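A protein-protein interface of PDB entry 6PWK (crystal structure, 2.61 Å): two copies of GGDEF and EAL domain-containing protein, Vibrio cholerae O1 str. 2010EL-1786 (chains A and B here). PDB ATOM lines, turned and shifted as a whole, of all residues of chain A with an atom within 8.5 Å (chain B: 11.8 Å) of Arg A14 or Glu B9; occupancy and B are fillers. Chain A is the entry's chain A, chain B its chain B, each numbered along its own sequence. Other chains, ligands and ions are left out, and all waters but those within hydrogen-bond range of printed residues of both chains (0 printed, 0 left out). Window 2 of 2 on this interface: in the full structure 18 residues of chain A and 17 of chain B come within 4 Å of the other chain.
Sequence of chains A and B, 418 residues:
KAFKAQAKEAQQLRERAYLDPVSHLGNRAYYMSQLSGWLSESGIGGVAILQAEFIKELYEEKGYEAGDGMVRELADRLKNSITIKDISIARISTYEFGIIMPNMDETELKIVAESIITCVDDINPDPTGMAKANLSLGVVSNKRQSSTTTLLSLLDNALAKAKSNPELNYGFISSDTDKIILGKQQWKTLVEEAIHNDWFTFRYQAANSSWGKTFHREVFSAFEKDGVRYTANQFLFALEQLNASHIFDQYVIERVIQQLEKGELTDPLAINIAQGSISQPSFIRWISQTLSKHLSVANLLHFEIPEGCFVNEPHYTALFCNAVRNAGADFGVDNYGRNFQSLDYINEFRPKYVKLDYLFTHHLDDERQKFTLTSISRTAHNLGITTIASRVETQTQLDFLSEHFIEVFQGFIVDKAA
Printed residues of chain A that touch a printed residue of chain B: Ala A10, Leu A13, Arg A14, Arg A16, Ala A17 and Tyr A18. Of the 19 printed residues of chain B, 7 touch a printed residue of chain A. Hydrophobic or aromatic side chains of chain B within 4 Å of the printed part of chain A: Leu B13, Ala B17, Tyr B18 and Ala B29.
CD1 of Leu B13 touches O of Ala A10 (3.7 Å). Arg B14 touches Leu A13 (N to CD2, 3.9 Å). Leu A13 touches Tyr B18 (CD1 to OH, 3.9 Å). Arg A14 touches Leu B13. CG of Arg A16 touches CB of Ala B17, 3.6 Å away. Arg A16 touches Ala B29 (CD to CB, 3.9 Å). CB of Arg B16 touches CB of Ala A17, 3.6 Å away. Ala B17 touches Ala A17.
The side-chain carboxylate (OE1) of Glu B9 lies within salt-bridge range of the guanidinium group (NH2) of Arg A14 (3.7 Å). The side-chain hydroxyl of Tyr A18 is in hydrogen-bond range of the guanidinium group of Arg B16 (2.8 Å).
Leu A13 touches Arg B14, and with the chains exchanged Arg A14 touches Leu B13. Leu A13 touches Tyr B18, but with the chains exchanged Tyr A18 does not touch Leu B13 (4.3 Å). Arg A14 touches Glu B9, but with the chains exchanged Glu A9 does not touch Arg B14 (6.9 Å). Ala A17 touches its own counterpart, Ala B17. Positions printed for both chains: 6, 7, 8, 9, 10, 11, 12, 13, 14, 15, 16, 17, 18 and 27. Of the 10 pairs that touch across the chains among the printed residues, 5 have their exchanged pair printed and touching as well.
Of chain B, only Glu B9 and Leu B13 come within 4 Å of Arg A14. Of chain A, only Arg A14 comes within 4 Å of Glu B9. No residue of chain B comes within 4 Å of Gln A11. Of chain B, only Arg B16 (3.6 Å) and Ala B17 (3.9 Å) come within 4 Å of Ala A17. Tyr A18 touches just one residue of chain B: Arg B16 (2.8 Å). No residue of chain B comes within 4 Å of Leu A19. Printed residues of chain A within 4 Å of Ala B29: Arg A16. Printed residues of chain A within 4 Å of Arg B16: Ala A17 (3.6 Å) and Tyr A18 (2.8 Å). Of the printed residues of chain B, Arg A16 touches Ala B17 (3.6 Å) and Ala B29 (3.9 Å). Lys B8 touches none of the printed residues of chain A. The nearest residue of chain B that does not touch Arg A14 is Ala B17 (6.1 Å).
The backbone carbonyl oxygen of Ala A17 is in hydrogen-bond range of the side-chain amide nitrogen of Asn A27. O of Tyr A18 is in hydrogen-bond range of N of Asn A27. OE2 of Glu B9 lies close to OE1 of Gln B6 (2.8 Å). O of Ala B17 lies within hydrogen-bond range of ND2 of Asn B27 (2.7 Å). The backbone carbonyl oxygen of Tyr B18 is in hydrogen-bond range of the backbone NH of Asn B27, at 3.0 Å. OD1 of Asn B27 is in hydrogen-bond range of N of Ala B29 (3.4 Å).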
ATOM      1  N   GLN A   6       6.558  20.559  -8.517  1.00  0.00           N
ATOM      2  CA  GLN A   6       5.107  20.453  -8.386  1.00  0.00           C
ATOM      3  C   GLN A   6       4.711  19.383  -7.374  1.00  0.00           C
ATOM      4  O   GLN A   6       3.876  19.624  -6.495  1.00  0.00           O
ATOM      5  CB  GLN A   6       4.482  20.152  -9.750  1.00  0.00           C
ATOM      6  CG  GLN A   6       2.967  20.068  -9.739  1.00  0.00           C
ATOM      7  CD  GLN A   6       2.307  21.414  -9.538  1.00  0.00           C
ATOM      8  OE1 GLN A   6       1.993  21.800  -8.413  1.00  0.00           O
ATOM      9  NE2 GLN A   6       2.081  22.134 -10.632  1.00  0.00           N
ATOM     10  N   ALA A   7       5.306  18.192  -7.483  1.00  0.00           N
ATOM     11  CA  ALA A   7       4.899  17.073  -6.638  1.00  0.00           C
ATOM     12  C   ALA A   7       5.119  17.380  -5.161  1.00  0.00           C
ATOM     13  O   ALA A   7       4.237  17.138  -4.329  1.00  0.00           O
ATOM     14  CB  ALA A   7       5.652  15.806  -7.048  1.00  0.00           C
ATOM     15  N   LYS A   8       6.287  17.923  -4.814  1.00  0.00           N
ATOM     16  CA  LYS A   8       6.544  18.268  -3.418  1.00  0.00           C
ATOM     17  C   LYS A   8       5.867  19.573  -3.015  1.00  0.00           C
ATOM     18  O   LYS A   8       5.457  19.716  -1.859  1.00  0.00           O
ATOM     19  CB  LYS A   8       8.050  18.325  -3.160  1.00  0.00           C
ATOM     20  CG  LYS A   8       8.602  17.006  -2.630  1.00  0.00           C
ATOM     21  CD  LYS A   8      10.037  16.753  -3.051  1.00  0.00           C
ATOM     22  CE  LYS A   8      10.469  15.355  -2.632  1.00  0.00           C
ATOM     23  NZ  LYS A   8      11.834  15.005  -3.114  1.00  0.00           N
ATOM     24  N   GLU A   9       5.718  20.523  -3.943  1.00  0.00           N
ATOM     25  CA  GLU A   9       4.929  21.715  -3.641  1.00  0.00           C
ATOM     26  C   GLU A   9       3.474  21.353  -3.379  1.00  0.00           C
ATOM     27  O   GLU A   9       2.811  21.980  -2.543  1.00  0.00           O
ATOM     28  CB  GLU A   9       5.023  22.726  -4.789  1.00  0.00           C
ATOM     29  CG  GLU A   9       4.125  23.943  -4.642  1.00  0.00           C
ATOM     30  CD  GLU A   9       4.610  24.904  -3.576  1.00  0.00           C
ATOM     31  OE1 GLU A   9       4.709  26.114  -3.867  1.00  0.00           O
ATOM     32  OE2 GLU A   9       4.905  24.449  -2.452  1.00  0.00           O
ATOM     33  N   ALA A  10       2.962  20.339  -4.081  1.00  0.00           N
ATOM     34  CA  ALA A  10       1.585  19.911  -3.861  1.00  0.00           C
ATOM     35  C   ALA A  10       1.387  19.400  -2.441  1.00  0.00           C
ATOM     36  O   ALA A  10       0.383  19.722  -1.793  1.00  0.00           O
ATOM     37  CB  ALA A  10       1.196  18.835  -4.875  1.00  0.00           C
ATOM     38  N   GLN A  11       2.334  18.607  -1.935  1.00  0.00           N
ATOM     39  CA  GLN A  11       2.187  18.056  -0.592  1.00  0.00           C
ATOM     40  C   GLN A  11       2.322  19.136   0.472  1.00  0.00           C
ATOM     41  O   GLN A  11       1.588  19.125   1.467  1.00  0.00           O
ATOM     42  CB  GLN A  11       3.213  16.944  -0.364  1.00  0.00           C
ATOM     43  CG  GLN A  11       3.078  16.239   0.982  1.00  0.00           C
ATOM     44  CD  GLN A  11       1.726  15.569   1.169  1.00  0.00           C
ATOM     45  OE1 GLN A  11       1.052  15.217   0.200  1.00  0.00           O
ATOM     46  NE2 GLN A  11       1.324  15.391   2.423  1.00  0.00           N
ATOM     47  N   GLN A  12       3.249  20.078   0.285  1.00  0.00           N
ATOM     48  CA  GLN A  12       3.378  21.174   1.241  1.00  0.00           C
ATOM     49  C   GLN A  12       2.159  22.088   1.200  1.00  0.00           C
ATOM     50  O   GLN A  12       1.711  22.579   2.243  1.00  0.00           O
ATOM     51  CB  GLN A  12       4.659  21.966   0.974  1.00  0.00           C
ATOM     52  CG  GLN A  12       5.885  21.404   1.681  1.00  0.00           C
ATOM     53  CD  GLN A  12       6.877  20.766   0.728  1.00  0.00           C
ATOM     54  OE1 GLN A  12       7.121  21.278  -0.363  1.00  0.00           O
ATOM     55  NE2 GLN A  12       7.455  19.643   1.139  1.00  0.00           N
ATOM     56  N   LEU A  13       1.609  22.328   0.008  1.00  0.00           N
ATOM     57  CA  LEU A  13       0.360  23.076  -0.082  1.00  0.00           C
ATOM     58  C   LEU A  13      -0.787  22.300   0.551  1.00  0.00           C
ATOM     59  O   LEU A  13      -1.636  22.880   1.238  1.00  0.00           O
ATOM     60  CB  LEU A  13       0.042  23.399  -1.543  1.00  0.00           C
ATOM     61  CG  LEU A  13       0.223  24.854  -1.980  1.00  0.00           C
ATOM     62  CD1 LEU A  13       1.617  25.351  -1.635  1.00  0.00           C
ATOM     63  CD2 LEU A  13      -0.048  24.994  -3.470  1.00  0.00           C
ATOM     64  N   ARG A  14      -0.822  20.983   0.334  1.00  0.00           N
ATOM     65  CA  ARG A  14      -1.864  20.157   0.932  1.00  0.00           C
ATOM     66  C   ARG A  14      -1.774  20.165   2.452  1.00  0.00           C
ATOM     67  O   ARG A  14      -2.799  20.239   3.141  1.00  0.00           O
ATOM     68  CB  ARG A  14      -1.771  18.728   0.397  1.00  0.00           C
ATOM     69  CG  ARG A  14      -2.771  17.768   1.016  1.00  0.00           C
ATOM     70  CD  ARG A  14      -2.601  16.369   0.458  1.00  0.00           C
ATOM     71  NE  ARG A  14      -2.597  16.372  -1.000  1.00  0.00           N
ATOM     72  CZ  ARG A  14      -3.686  16.521  -1.747  1.00  0.00           C
ATOM     73  NH1 ARG A  14      -4.868  16.686  -1.169  1.00  0.00           N
ATOM     74  NH2 ARG A  14      -3.593  16.512  -3.070  1.00  0.00           N
ATOM     75  N   GLU A  15      -0.558  20.090   2.998  1.00  0.00           N
ATOM     76  CA  GLU A  15      -0.412  20.096   4.451  1.00  0.00           C
ATOM     77  C   GLU A  15      -0.630  21.488   5.028  1.00  0.00           C
ATOM     78  O   GLU A  15      -1.114  21.621   6.157  1.00  0.00           O
ATOM     79  CB  GLU A  15       0.960  19.548   4.851  1.00  0.00           C
ATOM     80  CG  GLU A  15       2.129  20.479   4.576  1.00  0.00           C
ATOM     81  CD  GLU A  15       3.461  19.880   4.989  1.00  0.00           C
ATOM     82  OE1 GLU A  15       4.377  20.651   5.348  1.00  0.00           O
ATOM     83  OE2 GLU A  15       3.588  18.637   4.959  1.00  0.00           O
ATOM     84  N   ARG A  16      -0.289  22.536   4.276  1.00  0.00           N
ATOM     85  CA  ARG A  16      -0.567  23.886   4.751  1.00  0.00           C
ATOM     86  C   ARG A  16      -2.065  24.136   4.841  1.00  0.00           C
ATOM     87  O   ARG A  16      -2.538  24.794   5.773  1.00  0.00           O
ATOM     88  CB  ARG A  16       0.094  24.914   3.831  1.00  0.00           C
ATOM     89  CG  ARG A  16      -0.237  26.361   4.173  1.00  0.00           C
ATOM     90  CD  ARG A  16       0.243  26.725   5.567  1.00  0.00           C
ATOM     91  NE  ARG A  16       1.693  26.603   5.688  1.00  0.00           N
ATOM     92  CZ  ARG A  16       2.370  26.803   6.815  1.00  0.00           C
ATOM     93  NH1 ARG A  16       1.729  27.134   7.927  1.00  0.00           N
ATOM     94  NH2 ARG A  16       3.688  26.669   6.830  1.00  0.00           N
ATOM     95  N   ALA A  17      -2.828  23.600   3.889  1.00  0.00           N
ATOM     96  CA  ALA A  17      -4.260  23.868   3.847  1.00  0.00           C
ATOM     97  C   ALA A  17      -5.029  23.036   4.866  1.00  0.00           C
ATOM     98  O   ALA A  17      -5.994  23.526   5.464  1.00  0.00           O
ATOM     99  CB  ALA A  17      -4.795  23.612   2.438  1.00  0.00           C
ATOM    100  N   TYR A  18      -4.616  21.784   5.089  1.00  0.00           N
ATOM    101  CA  TYR A  18      -5.425  20.835   5.843  1.00  0.00           C
ATOM    102  C   TYR A  18      -4.760  20.265   7.090  1.00  0.00           C
ATOM    103  O   TYR A  18      -5.425  19.535   7.832  1.00  0.00           O
ATOM    104  CB  TYR A  18      -5.851  19.668   4.941  1.00  0.00           C
ATOM    105  CG  TYR A  18      -6.775  20.065   3.811  1.00  0.00           C
ATOM    106  CD1 TYR A  18      -7.772  21.014   4.007  1.00  0.00           C
ATOM    107  CD2 TYR A  18      -6.646  19.501   2.549  1.00  0.00           C
ATOM    108  CE1 TYR A  18      -8.617  21.382   2.978  1.00  0.00           C
ATOM    109  CE2 TYR A  18      -7.487  19.863   1.515  1.00  0.00           C
ATOM    110  CZ  TYR A  18      -8.470  20.805   1.735  1.00  0.00           C
ATOM    111  OH  TYR A  18      -9.310  21.170   0.707  1.00  0.00           O
ATOM    112  N   LEU A  19      -3.489  20.560   7.349  1.00  0.00           N
ATOM    113  CA  LEU A  19      -2.786  19.993   8.497  1.00  0.00           C
ATOM    114  C   LEU A  19      -2.466  21.083   9.510  1.00  0.00           C
ATOM    115  O   LEU A  19      -1.915  22.131   9.152  1.00  0.00           O
ATOM    116  CB  LEU A  19      -1.497  19.287   8.071  1.00  0.00           C
ATOM    117  CG  LEU A  19      -0.771  18.512   9.174  1.00  0.00           C
ATOM    118  CD1 LEU A  19      -1.405  17.143   9.372  1.00  0.00           C
ATOM    119  CD2 LEU A  19       0.715  18.384   8.870  1.00  0.00           C
ATOM    120  N   ASP A  20      -2.809  20.830  10.769  1.00  0.00           N
ATOM    121  CA  ASP A  20      -2.456  21.740  11.854  1.00  0.00           C
ATOM    122  C   ASP A  20      -1.025  21.466  12.301  1.00  0.00           C
ATOM    123  O   ASP A  20      -0.716  20.334  12.690  1.00  0.00           O
ATOM    124  CB  ASP A  20      -3.418  21.572  13.024  1.00  0.00           C
ATOM    125  CG  ASP A  20      -2.951  22.296  14.271  1.00  0.00           C
ATOM    126  OD1 ASP A  20      -2.943  23.546  14.270  1.00  0.00           O
ATOM    127  OD2 ASP A  20      -2.591  21.615  15.254  1.00  0.00           O
ATOM    128  N   GLY A  26      -5.308  16.662  11.257  1.00  0.00           N
ATOM    129  CA  GLY A  26      -6.074  17.515  10.371  1.00  0.00           C
ATOM    130  C   GLY A  26      -6.568  18.752  11.096  1.00  0.00           C
ATOM    131  O   GLY A  26      -6.857  18.723  12.292  1.00  0.00           O
ATOM    132  N   ASN A  27      -6.639  19.860  10.368  1.00  0.00           N
ATOM    133  CA  ASN A  27      -7.136  21.097  10.952  1.00  0.00           C
ATOM    134  C   ASN A  27      -8.662  21.118  10.858  1.00  0.00           C
ATOM    135  O   ASN A  27      -9.303  20.113  10.540  1.00  0.00           O
ATOM    136  CB  ASN A  27      -6.487  22.310  10.283  1.00  0.00           C
ATOM    137  CG  ASN A  27      -6.761  22.384   8.793  1.00  0.00           C
ATOM    138  OD1 ASN A  27      -7.539  21.604   8.245  1.00  0.00           O
ATOM    139  ND2 ASN A  27      -6.121  23.339   8.129  1.00  0.00           N
ATOM    140  N   TYR A  30      -9.971  20.508   7.256  1.00  0.00           N
ATOM    141  CA  TYR A  30      -9.904  19.084   6.947  1.00  0.00           C
ATOM    142  C   TYR A  30     -11.083  18.340   7.555  1.00  0.00           C
ATOM    143  O   TYR A  30     -11.654  17.441   6.925  1.00  0.00           O
ATOM    144  CB  TYR A  30      -8.582  18.501   7.453  1.00  0.00           C
ATOM    145  CG  TYR A  30      -8.564  16.992   7.594  1.00  0.00           C
ATOM    146  CD1 TYR A  30      -8.187  16.178   6.533  1.00  0.00           C
ATOM    147  CD2 TYR A  30      -8.907  16.381   8.797  1.00  0.00           C
ATOM    148  CE1 TYR A  30      -8.164  14.801   6.662  1.00  0.00           C
ATOM    149  CE2 TYR A  30      -8.889  15.007   8.933  1.00  0.00           C
ATOM    150  CZ  TYR A  30      -8.515  14.221   7.864  1.00  0.00           C
ATOM    151  OH  TYR A  30      -8.494  12.852   7.995  1.00  0.00           O
ATOM    152  N   ALA B   2      -5.698  16.979 -18.505  1.00  0.00           N
ATOM    153  CA  ALA B   2      -4.904  16.766 -17.301  1.00  0.00           C
ATOM    154  C   ALA B   2      -4.148  18.034 -16.914  1.00  0.00           C
ATOM    155  O   ALA B   2      -3.869  18.263 -15.736  1.00  0.00           O
ATOM    156  CB  ALA B   2      -3.937  15.612 -17.500  1.00  0.00           C
ATOM    157  N   PHE B   3      -3.814  18.854 -17.913  1.00  0.00           N
ATOM    158  CA  PHE B   3      -3.128  20.112 -17.638  1.00  0.00           C
ATOM    159  C   PHE B   3      -4.058  21.101 -16.945  1.00  0.00           C
ATOM    160  O   PHE B   3      -3.694  21.701 -15.927  1.00  0.00           O
ATOM    161  CB  PHE B   3      -2.573  20.708 -18.933  1.00  0.00           C
ATOM    162  CG  PHE B   3      -1.867  22.022 -18.743  1.00  0.00           C
ATOM    163  CD1 PHE B   3      -0.546  22.058 -18.326  1.00  0.00           C
ATOM    164  CD2 PHE B   3      -2.521  23.220 -18.984  1.00  0.00           C
ATOM    165  CE1 PHE B   3       0.109  23.261 -18.149  1.00  0.00           C
ATOM    166  CE2 PHE B   3      -1.871  24.428 -18.808  1.00  0.00           C
ATOM    167  CZ  PHE B   3      -0.553  24.448 -18.391  1.00  0.00           C
ATOM    168  N   LYS B   4      -5.264  21.287 -17.488  1.00  0.00           N
ATOM    169  CA  LYS B   4      -6.234  22.163 -16.843  1.00  0.00           C
ATOM    170  C   LYS B   4      -6.687  21.599 -15.504  1.00  0.00           C
ATOM    171  O   LYS B   4      -7.002  22.364 -14.584  1.00  0.00           O
ATOM    172  CB  LYS B   4      -7.435  22.389 -17.762  1.00  0.00           C
ATOM    173  N   ALA B   5      -6.720  20.271 -15.373  1.00  0.00           N
ATOM    174  CA  ALA B   5      -7.106  19.657 -14.108  1.00  0.00           C
ATOM    175  C   ALA B   5      -6.043  19.888 -13.043  1.00  0.00           C
ATOM    176  O   ALA B   5      -6.360  20.251 -11.904  1.00  0.00           O
ATOM    177  CB  ALA B   5      -7.357  18.162 -14.307  1.00  0.00           C
ATOM    178  N   GLN B   6      -4.773  19.686 -13.399  1.00  0.00           N
ATOM    179  CA  GLN B   6      -3.695  19.900 -12.440  1.00  0.00           C
ATOM    180  C   GLN B   6      -3.633  21.355 -11.990  1.00  0.00           C
ATOM    181  O   GLN B   6      -3.319  21.639 -10.828  1.00  0.00           O
ATOM    182  CB  GLN B   6      -2.362  19.474 -13.057  1.00  0.00           C
ATOM    183  CG  GLN B   6      -1.234  19.309 -12.050  1.00  0.00           C
ATOM    184  CD  GLN B   6      -1.390  18.055 -11.209  1.00  0.00           C
ATOM    185  OE1 GLN B   6      -1.176  18.073  -9.996  1.00  0.00           O
ATOM    186  NE2 GLN B   6      -1.767  16.955 -11.853  1.00  0.00           N
ATOM    187  N   ALA B   7      -3.925  22.292 -12.898  1.00  0.00           N
ATOM    188  CA  ALA B   7      -3.893  23.706 -12.539  1.00  0.00           C
ATOM    189  C   ALA B   7      -5.005  24.054 -11.557  1.00  0.00           C
ATOM    190  O   ALA B   7      -4.808  24.877 -10.656  1.00  0.00           O
ATOM    191  CB  ALA B   7      -3.998  24.567 -13.797  1.00  0.00           C
ATOM    192  N   LYS B   8      -6.181  23.440 -11.719  1.00  0.00           N
ATOM    193  CA  LYS B   8      -7.280  23.683 -10.790  1.00  0.00           C
ATOM    194  C   LYS B   8      -6.985  23.091  -9.418  1.00  0.00           C
ATOM    195  O   LYS B   8      -7.240  23.733  -8.393  1.00  0.00           O
ATOM    196  CB  LYS B   8      -8.581  23.112 -11.347  1.00  0.00           C
ATOM    197  CG  LYS B   8      -9.298  24.022 -12.326  1.00  0.00           C
ATOM    198  CD  LYS B   8     -10.462  23.300 -12.987  1.00  0.00           C
ATOM    199  CE  LYS B   8     -11.182  24.195 -13.981  1.00  0.00           C
ATOM    200  NZ  LYS B   8     -12.145  23.421 -14.813  1.00  0.00           N
ATOM    201  N   GLU B   9      -6.458  21.864  -9.380  1.00  0.00           N
ATOM    202  CA  GLU B   9      -6.120  21.244  -8.103  1.00  0.00           C
ATOM    203  C   GLU B   9      -5.059  22.048  -7.365  1.00  0.00           C
ATOM    204  O   GLU B   9      -5.160  22.260  -6.150  1.00  0.00           O
ATOM    205  CB  GLU B   9      -5.644  19.809  -8.322  1.00  0.00           C
ATOM    206  CG  GLU B   9      -5.125  19.135  -7.062  1.00  0.00           C
ATOM    207  CD  GLU B   9      -3.747  18.532  -7.247  1.00  0.00           C
ATOM    208  OE1 GLU B   9      -3.465  17.487  -6.627  1.00  0.00           O
ATOM    209  OE2 GLU B   9      -2.946  19.106  -8.016  1.00  0.00           O
ATOM    210  N   ALA B  10      -4.032  22.507  -8.084  1.00  0.00           N
ATOM    211  CA  ALA B  10      -2.995  23.315  -7.454  1.00  0.00           C
ATOM    212  C   ALA B  10      -3.536  24.674  -7.029  1.00  0.00           C
ATOM    213  O   ALA B  10      -3.197  25.170  -5.948  1.00  0.00           O
ATOM    214  CB  ALA B  10      -1.811  23.480  -8.406  1.00  0.00           C
ATOM    215  N   GLN B  11      -4.385  25.286  -7.859  1.00  0.00           N
ATOM    216  CA  GLN B  11      -4.918  26.603  -7.524  1.00  0.00           C
ATOM    217  C   GLN B  11      -5.870  26.530  -6.336  1.00  0.00           C
ATOM    218  O   GLN B  11      -5.842  27.401  -5.459  1.00  0.00           O
ATOM    219  CB  GLN B  11      -5.618  27.214  -8.737  1.00  0.00           C
ATOM    220  CG  GLN B  11      -6.062  28.656  -8.539  1.00  0.00           C
ATOM    221  CD  GLN B  11      -4.895  29.610  -8.340  1.00  0.00           C
ATOM    222  OE1 GLN B  11      -3.762  29.316  -8.723  1.00  0.00           O
ATOM    223  NE2 GLN B  11      -5.171  30.760  -7.736  1.00  0.00           N
ATOM    224  N   GLN B  12      -6.718  25.501  -6.287  1.00  0.00           N
ATOM    225  CA  GLN B  12      -7.618  25.346  -5.150  1.00  0.00           C
ATOM    226  C   GLN B  12      -6.849  25.008  -3.879  1.00  0.00           C
ATOM    227  O   GLN B  12      -7.158  25.535  -2.805  1.00  0.00           O
ATOM    228  CB  GLN B  12      -8.674  24.283  -5.452  1.00  0.00           C
ATOM    229  CG  GLN B  12      -9.784  24.770  -6.370  1.00  0.00           C
ATOM    230  CD  GLN B  12     -10.682  23.648  -6.852  1.00  0.00           C
ATOM    231  OE1 GLN B  12     -10.332  22.471  -6.753  1.00  0.00           O
ATOM    232  NE2 GLN B  12     -11.847  24.007  -7.380  1.00  0.00           N
ATOM    233  N   LEU B  13      -5.841  24.135  -3.978  1.00  0.00           N
ATOM    234  CA  LEU B  13      -4.956  23.898  -2.840  1.00  0.00           C
ATOM    235  C   LEU B  13      -4.288  25.192  -2.396  1.00  0.00           C
ATOM    236  O   LEU B  13      -4.215  25.490  -1.198  1.00  0.00           O
ATOM    237  CB  LEU B  13      -3.904  22.847  -3.198  1.00  0.00           C
ATOM    238  CG  LEU B  13      -4.198  21.391  -2.836  1.00  0.00           C
ATOM    239  CD1 LEU B  13      -2.976  20.522  -3.094  1.00  0.00           C
ATOM    240  CD2 LEU B  13      -4.643  21.277  -1.385  1.00  0.00           C
ATOM    241  N   ARG B  14      -3.790  25.974  -3.358  1.00  0.00           N
ATOM    242  CA  ARG B  14      -3.223  27.278  -3.035  1.00  0.00           C
ATOM    243  C   ARG B  14      -4.270  28.207  -2.439  1.00  0.00           C
ATOM    244  O   ARG B  14      -3.950  29.029  -1.574  1.00  0.00           O
ATOM    245  CB  ARG B  14      -2.613  27.903  -4.290  1.00  0.00           C
ATOM    246  CG  ARG B  14      -1.939  29.242  -4.057  1.00  0.00           C
ATOM    247  CD  ARG B  14      -1.422  29.832  -5.356  1.00  0.00           C
ATOM    248  NE  ARG B  14      -0.258  30.682  -5.130  1.00  0.00           N
ATOM    249  CZ  ARG B  14      -0.322  31.966  -4.790  1.00  0.00           C
ATOM    250  NH1 ARG B  14      -1.499  32.557  -4.634  1.00  0.00           N
ATOM    251  NH2 ARG B  14       0.793  32.658  -4.605  1.00  0.00           N
ATOM    252  N   GLU B  15      -5.522  28.087  -2.884  1.00  0.00           N
ATOM    253  CA  GLU B  15      -6.579  28.948  -2.367  1.00  0.00           C
ATOM    254  C   GLU B  15      -6.918  28.601  -0.922  1.00  0.00           C
ATOM    255  O   GLU B  15      -7.114  29.496  -0.093  1.00  0.00           O
ATOM    256  CB  GLU B  15      -7.819  28.844  -3.254  1.00  0.00           C
ATOM    257  CG  GLU B  15      -8.872  29.906  -2.987  1.00  0.00           C
ATOM    258  CD  GLU B  15     -10.098  29.737  -3.864  1.00  0.00           C
ATOM    259  OE1 GLU B  15     -10.297  28.626  -4.399  1.00  0.00           O
ATOM    260  OE2 GLU B  15     -10.861  30.713  -4.020  1.00  0.00           O
ATOM    261  N   ARG B  16      -6.992  27.310  -0.599  1.00  0.00           N
ATOM    262  CA  ARG B  16      -7.252  26.920   0.784  1.00  0.00           C
ATOM    263  C   ARG B  16      -6.096  27.294   1.700  1.00  0.00           C
ATOM    264  O   ARG B  16      -6.311  27.605   2.877  1.00  0.00           O
ATOM    265  CB  ARG B  16      -7.516  25.418   0.868  1.00  0.00           C
ATOM    266  CG  ARG B  16      -8.551  24.904  -0.116  1.00  0.00           C
ATOM    267  CD  ARG B  16      -9.891  25.580   0.089  1.00  0.00           C
ATOM    268  NE  ARG B  16     -10.445  25.281   1.404  1.00  0.00           N
ATOM    269  CZ  ARG B  16     -11.096  24.161   1.700  1.00  0.00           C
ATOM    270  NH1 ARG B  16     -11.269  23.229   0.773  1.00  0.00           N
ATOM    271  NH2 ARG B  16     -11.569  23.972   2.924  1.00  0.00           N
ATOM    272  N   ALA B  17      -4.869  27.282   1.181  1.00  0.00           N
ATOM    273  CA  ALA B  17      -3.705  27.489   2.030  1.00  0.00           C
ATOM    274  C   ALA B  17      -3.418  28.969   2.255  1.00  0.00           C
ATOM    275  O   ALA B  17      -2.985  29.357   3.345  1.00  0.00           O
ATOM    276  CB  ALA B  17      -2.485  26.800   1.418  1.00  0.00           C
ATOM    277  N   TYR B  18      -3.658  29.808   1.246  1.00  0.00           N
ATOM    278  CA  TYR B  18      -3.167  31.178   1.260  1.00  0.00           C
ATOM    279  C   TYR B  18      -4.251  32.247   1.225  1.00  0.00           C
ATOM    280  O   TYR B  18      -3.912  33.435   1.210  1.00  0.00           O
ATOM    281  CB  TYR B  18      -2.210  31.404   0.080  1.00  0.00           C
ATOM    282  CG  TYR B  18      -0.922  30.620   0.169  1.00  0.00           C
ATOM    283  CD1 TYR B  18      -0.287  30.424   1.389  1.00  0.00           C
ATOM    284  CD2 TYR B  18      -0.341  30.074  -0.968  1.00  0.00           C
ATOM    285  CE1 TYR B  18       0.893  29.709   1.473  1.00  0.00           C
ATOM    286  CE2 TYR B  18       0.837  29.356  -0.893  1.00  0.00           C
ATOM    287  CZ  TYR B  18       1.450  29.176   0.329  1.00  0.00           C
ATOM    288  OH  TYR B  18       2.624  28.462   0.406  1.00  0.00           O
ATOM    289  N   ASN B  27      -3.635  35.253   3.630  1.00  0.00           N
ATOM    290  CA  ASN B  27      -3.607  35.060   5.070  1.00  0.00           C
ATOM    291  C   ASN B  27      -2.180  35.267   5.576  1.00  0.00           C
ATOM    292  O   ASN B  27      -1.309  35.764   4.857  1.00  0.00           O
ATOM    293  CB  ASN B  27      -4.171  33.687   5.441  1.00  0.00           C
ATOM    294  CG  ASN B  27      -3.398  32.539   4.816  1.00  0.00           C
ATOM    295  OD1 ASN B  27      -2.371  32.735   4.168  1.00  0.00           O
ATOM    296  ND2 ASN B  27      -3.893  31.323   5.021  1.00  0.00           N
ATOM    297  N   ALA B  29       0.109  32.958   6.415  1.00  0.00           N
ATOM    298  CA  ALA B  29       1.053  32.068   5.747  1.00  0.00           C
ATOM    299  C   ALA B  29       1.428  32.590   4.366  1.00  0.00           C
ATOM    300  O   ALA B  29       2.582  32.460   3.938  1.00  0.00           O
ATOM    301  CB  ALA B  29       0.466  30.661   5.646  1.00  0.00           C
